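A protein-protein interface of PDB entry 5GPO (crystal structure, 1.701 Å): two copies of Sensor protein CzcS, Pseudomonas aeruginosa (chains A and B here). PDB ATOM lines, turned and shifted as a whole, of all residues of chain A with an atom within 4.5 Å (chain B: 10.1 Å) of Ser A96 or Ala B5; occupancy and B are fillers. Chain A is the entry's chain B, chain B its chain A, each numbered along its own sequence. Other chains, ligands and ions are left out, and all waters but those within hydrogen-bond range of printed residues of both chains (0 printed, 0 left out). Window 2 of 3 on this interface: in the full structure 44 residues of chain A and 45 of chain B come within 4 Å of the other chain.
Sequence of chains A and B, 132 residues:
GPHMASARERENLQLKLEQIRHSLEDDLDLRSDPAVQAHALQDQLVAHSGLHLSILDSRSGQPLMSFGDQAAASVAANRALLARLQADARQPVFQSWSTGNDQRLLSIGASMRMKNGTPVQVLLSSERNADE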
ATOM      1  N   PHE A  94      17.997  28.184 -15.379  1.00  0.00           N
ATOM      2  CA  PHE A  94      18.832  27.880 -14.232  1.00  0.00           C
ATOM      3  C   PHE A  94      19.363  26.464 -14.343  1.00  0.00           C
ATOM      4  O   PHE A  94      18.694  25.559 -14.851  1.00  0.00           O
ATOM      5  CB  PHE A  94      18.064  28.017 -12.916  1.00  0.00           C
ATOM      6  CG  PHE A  94      17.912  29.427 -12.452  1.00  0.00           C
ATOM      7  CD1 PHE A  94      18.899  30.017 -11.674  1.00  0.00           C
ATOM      8  CD2 PHE A  94      16.788  30.164 -12.787  1.00  0.00           C
ATOM      9  CE1 PHE A  94      18.765  31.332 -11.234  1.00  0.00           C
ATOM     10  CE2 PHE A  94      16.643  31.472 -12.346  1.00  0.00           C
ATOM     11  CZ  PHE A  94      17.640  32.057 -11.571  1.00  0.00           C
ATOM     12  N   GLN A  95      20.574  26.271 -13.840  1.00  0.00           N
ATOM     13  CA  GLN A  95      21.184  24.955 -13.878  1.00  0.00           C
ATOM     14  C   GLN A  95      21.987  24.753 -12.612  1.00  0.00           C
ATOM     15  O   GLN A  95      22.877  25.552 -12.312  1.00  0.00           O
ATOM     16  CB  GLN A  95      22.080  24.808 -15.098  1.00  0.00           C
ATOM     17  CG  GLN A  95      22.756  23.468 -15.170  1.00  0.00           C
ATOM     18  CD  GLN A  95      23.916  23.506 -16.117  1.00  0.00           C
ATOM     19  OE1 GLN A  95      24.907  24.211 -15.873  1.00  0.00           O
ATOM     20  NE2 GLN A  95      23.803  22.779 -17.218  1.00  0.00           N
ATOM     21  N   SER A  96      21.660  23.707 -11.865  1.00  0.00           N
ATOM     22  CA  SER A  96      22.557  23.214 -10.839  1.00  0.00           C
ATOM     23  C   SER A  96      23.344  22.054 -11.424  1.00  0.00           C
ATOM     24  O   SER A  96      22.877  21.363 -12.334  1.00  0.00           O
ATOM     25  CB  SER A  96      21.797  22.793  -9.582  1.00  0.00           C
ATOM     26  OG  SER A  96      21.000  23.865  -9.104  1.00  0.00           O
ATOM     27  N   TRP A  97      24.568  21.878 -10.935  1.00  0.00           N
ATOM     28  CA  TRP A  97      25.473  20.894 -11.508  1.00  0.00           C
ATOM     29  C   TRP A  97      26.442  20.451 -10.428  1.00  0.00           C
ATOM     30  O   TRP A  97      26.896  21.271  -9.627  1.00  0.00           O
ATOM     31  CB  TRP A  97      26.230  21.481 -12.706  1.00  0.00           C
ATOM     32  CG  TRP A  97      26.838  20.464 -13.631  1.00  0.00           C
ATOM     33  CD1 TRP A  97      28.075  19.885 -13.518  1.00  0.00           C
ATOM     34  CD2 TRP A  97      26.244  19.919 -14.809  1.00  0.00           C
ATOM     35  NE1 TRP A  97      28.281  19.015 -14.561  1.00  0.00           N
ATOM     36  CE2 TRP A  97      27.175  19.013 -15.366  1.00  0.00           C
ATOM     37  CE3 TRP A  97      25.015  20.108 -15.452  1.00  0.00           C
ATOM     38  CZ2 TRP A  97      26.914  18.295 -16.537  1.00  0.00           C
ATOM     39  CZ3 TRP A  97      24.756  19.400 -16.622  1.00  0.00           C
ATOM     40  CH2 TRP A  97      25.703  18.499 -17.150  1.00  0.00           C
ATOM     41  N   LEU A 105      27.859  23.606  -8.665  1.00  0.00           N
ATOM     42  CA  LEU A 105      27.797  24.869  -9.387  1.00  0.00           C
ATOM     43  C   LEU A 105      26.352  25.293  -9.571  1.00  0.00           C
ATOM     44  O   LEU A 105      25.456  24.453  -9.701  1.00  0.00           O
ATOM     45  CB  LEU A 105      28.446  24.760 -10.773  1.00  0.00           C
ATOM     46  CG  LEU A 105      29.907  24.340 -10.738  1.00  0.00           C
ATOM     47  CD1 LEU A 105      30.405  24.129 -12.151  1.00  0.00           C
ATOM     48  CD2 LEU A 105      30.733  25.404 -10.011  1.00  0.00           C
ATOM     49  N   LEU A 106      26.133  26.603  -9.586  1.00  0.00           N
ATOM     50  CA  LEU A 106      24.859  27.180  -9.992  1.00  0.00           C
ATOM     51  C   LEU A 106      25.126  28.140 -11.141  1.00  0.00           C
ATOM     52  O   LEU A 106      25.963  29.039 -11.024  1.00  0.00           O
ATOM     53  CB  LEU A 106      24.153  27.896  -8.838  1.00  0.00           C
ATOM     54  CG  LEU A 106      22.822  28.534  -9.271  1.00  0.00           C
ATOM     55  CD1 LEU A 106      21.866  27.505  -9.878  1.00  0.00           C
ATOM     56  CD2 LEU A 106      22.142  29.294  -8.114  1.00  0.00           C
ATOM     57  N   ARG A 128      28.760  27.394  -5.591  1.00  0.00           N
ATOM     58  CA  ARG A 128      27.800  27.374  -4.487  1.00  0.00           C
ATOM     59  C   ARG A 128      28.506  27.212  -3.143  1.00  0.00           C
ATOM     60  O   ARG A 128      29.591  27.754  -2.930  1.00  0.00           O
ATOM     61  CB  ARG A 128      26.776  26.247  -4.672  1.00  0.00           C
ATOM     62  CG  ARG A 128      25.777  26.477  -5.800  1.00  0.00           C
ATOM     63  CD  ARG A 128      24.726  25.377  -5.835  1.00  0.00           C
ATOM     64  NE  ARG A 128      23.970  25.309  -4.585  1.00  0.00           N
ATOM     65  CZ  ARG A 128      23.028  24.405  -4.326  1.00  0.00           C
ATOM     66  NH1 ARG A 128      22.720  23.482  -5.226  1.00  0.00           N
ATOM     67  NH2 ARG A 128      22.390  24.421  -3.163  1.00  0.00           N
ATOM     68  N   ALA B   5      19.395  24.048  -6.215  1.00  0.00           N
ATOM     69  CA  ALA B   5      19.767  25.364  -5.708  1.00  0.00           C
ATOM     70  C   ALA B   5      18.565  26.084  -5.094  1.00  0.00           C
ATOM     71  O   ALA B   5      17.441  25.985  -5.597  1.00  0.00           O
ATOM     72  CB  ALA B   5      20.382  26.202  -6.819  1.00  0.00           C
ATOM     73  N   SER B   6      18.818  26.820  -4.011  1.00  0.00           N
ATOM     74  CA  SER B   6      17.746  27.386  -3.208  1.00  0.00           C
ATOM     75  C   SER B   6      17.111  28.584  -3.913  1.00  0.00           C
ATOM     76  O   SER B   6      17.604  29.085  -4.928  1.00  0.00           O
ATOM     77  CB  SER B   6      18.266  27.809  -1.834  1.00  0.00           C
ATOM     78  OG  SER B   6      18.999  29.024  -1.906  1.00  0.00           O
ATOM     79  N   ALA B   7      15.996  29.045  -3.342  1.00  0.00           N
ATOM     80  CA  ALA B   7      15.301  30.208  -3.880  1.00  0.00           C
ATOM     81  C   ALA B   7      16.178  31.451  -3.840  1.00  0.00           C
ATOM     82  O   ALA B   7      16.199  32.232  -4.799  1.00  0.00           O
ATOM     83  CB  ALA B   7      14.008  30.451  -3.103  1.00  0.00           C
ATOM     84  N   ARG B   8      16.909  31.651  -2.739  1.00  0.00           N
ATOM     85  CA  ARG B   8      17.693  32.875  -2.581  1.00  0.00           C
ATOM     86  C   ARG B   8      18.938  32.864  -3.456  1.00  0.00           C
ATOM     87  O   ARG B   8      19.320  33.904  -4.006  1.00  0.00           O
ATOM     88  CB  ARG B   8      18.084  33.073  -1.118  1.00  0.00           C
ATOM     89  CG  ARG B   8      18.657  34.459  -0.837  1.00  0.00           C
ATOM     90  N   GLU B   9      19.603  31.710  -3.563  1.00  0.00           N
ATOM     91  CA  GLU B   9      20.726  31.570  -4.488  1.00  0.00           C
ATOM     92  C   GLU B   9      20.306  31.889  -5.920  1.00  0.00           C
ATOM     93  O   GLU B   9      21.022  32.588  -6.647  1.00  0.00           O
ATOM     94  CB  GLU B   9      21.299  30.151  -4.417  1.00  0.00           C
ATOM     95  CG  GLU B   9      22.048  29.784  -3.147  1.00  0.00           C
ATOM     96  CD  GLU B   9      22.546  28.338  -3.175  1.00  0.00           C
ATOM     97  OE1 GLU B   9      21.712  27.417  -3.302  1.00  0.00           O
ATOM     98  OE2 GLU B   9      23.771  28.121  -3.087  1.00  0.00           O
ATOM     99  N   ARG B  10      19.155  31.357  -6.357  1.00  0.00           N
ATOM    100  CA  ARG B  10      18.698  31.642  -7.712  1.00  0.00           C
ATOM    101  C   ARG B  10      18.378  33.119  -7.867  1.00  0.00           C
ATOM    102  O   ARG B  10      18.747  33.740  -8.869  1.00  0.00           O
ATOM    103  CB  ARG B  10      17.481  30.786  -8.059  1.00  0.00           C
ATOM    104  CG  ARG B  10      17.774  29.295  -8.140  1.00  0.00           C
ATOM    105  CD  ARG B  10      16.601  28.559  -8.784  1.00  0.00           C
ATOM    106  NE  ARG B  10      15.313  28.878  -8.161  1.00  0.00           N
ATOM    107  CZ  ARG B  10      14.746  28.143  -7.207  1.00  0.00           C
ATOM    108  NH1 ARG B  10      15.357  27.050  -6.764  1.00  0.00           N
ATOM    109  NH2 ARG B  10      13.571  28.495  -6.692  1.00  0.00           N
ATOM    110  N   GLU B  11      17.712  33.704  -6.865  1.00  0.00           N
ATOM    111  CA  GLU B  11      17.391  35.128  -6.906  1.00  0.00           C
ATOM    112  C   GLU B  11      18.658  35.965  -7.063  1.00  0.00           C
ATOM    113  O   GLU B  11      18.706  36.892  -7.878  1.00  0.00           O
ATOM    114  CB  GLU B  11      16.644  35.529  -5.628  1.00  0.00           C
ATOM    115  CG  GLU B  11      16.170  36.977  -5.622  1.00  0.00           C
ATOM    116  CD  GLU B  11      15.600  37.422  -4.278  1.00  0.00           C
ATOM    117  OE1 GLU B  11      15.524  38.649  -4.055  1.00  0.00           O
ATOM    118  OE2 GLU B  11      15.229  36.554  -3.452  1.00  0.00           O
ATOM    119  N   ASN B  12      19.685  35.639  -6.283  1.00  0.00           N
ATOM    120  CA  ASN B  12      20.927  36.408  -6.315  1.00  0.00           C
ATOM    121  C   ASN B  12      21.639  36.296  -7.663  1.00  0.00           C
ATOM    122  O   ASN B  12      22.185  37.282  -8.164  1.00  0.00           O
ATOM    123  CB  ASN B  12      21.835  35.951  -5.177  1.00  0.00           C
ATOM    124  CG  ASN B  12      21.342  36.425  -3.813  1.00  0.00           C
ATOM    125  OD1 ASN B  12      20.603  37.401  -3.732  1.00  0.00           O
ATOM    126  ND2 ASN B  12      21.763  35.750  -2.745  1.00  0.00           N
ATOM    127  N   LEU B  13      21.644  35.110  -8.274  1.00  0.00           N
ATOM    128  CA  LEU B  13      22.300  34.992  -9.575  1.00  0.00           C
ATOM    129  C   LEU B  13      21.495  35.700 -10.663  1.00  0.00           C
ATOM    130  O   LEU B  13      22.070  36.249 -11.605  1.00  0.00           O
ATOM    131  CB  LEU B  13      22.504  33.512  -9.927  1.00  0.00           C
ATOM    132  CG  LEU B  13      23.735  33.157 -10.761  1.00  0.00           C
ATOM    133  CD1 LEU B  13      25.006  33.540 -10.042  1.00  0.00           C
ATOM    134  CD2 LEU B  13      23.731  31.658 -11.096  1.00  0.00           C
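N of Ala B5 is in hydrogen-bond range of OG of Ser A96 (3.3 Å). The side-chain carboxylate (OE1) of Glu B9 lies within salt-bridge range of the guanidinium group (NH2) of Arg A128, 3.1 Å away.
N of Ser B6 is in hydrogen-bond range of OE1 of Glu B9 (3.0 Å). NH1 of Arg B10 is in hydrogen-bond range of O of Ala B5 (2.6 Å).
Among the printed residues, merely in contact across the chains: Phe A94 with Arg B10, Leu A106 with Leu B13, Arg A128 with Ala B5, Leu A106 with Ala B5 and Leu A106 with Glu B9.
Gln A95 touches none of the printed residues of chain B. Of the printed residues of chain A, Glu B9 touches Leu A106 (3.8 Å) and Arg A128 (3.1 Å). Of the printed residues of chain B, Phe A94 touches Arg B10 (3.4 Å). Of the printed residues of chain A, Arg B10 touches Phe A94 (3.4 Å). Printed residues of chain B within 4 Å of Leu A106: Ala B5, Glu B9 and Leu B13. Of the printed residues of chain A, Leu B13 touches Leu A106 (3.4 Å). The nearest residue of chain B that does not touch Ser A96 is Ser B6 (6.3 Å). The nearest printed residue of chain A that does not touch Ala B5 is Gln A95 (6.1 Å).
Printed residues of chain A that touch a printed residue of chain B: Phe A94, Ser A96, Leu A106 and Arg A128. Of the 9 printed residues of chain B, 4 touch a printed residue of chain A. Among the printed residues, 7 pairs touch across the chains.
No position is printed for both chains. Of the 7 pairs that touch across the chains among the printed residues, none has its exchanged pair printed and touching as well.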
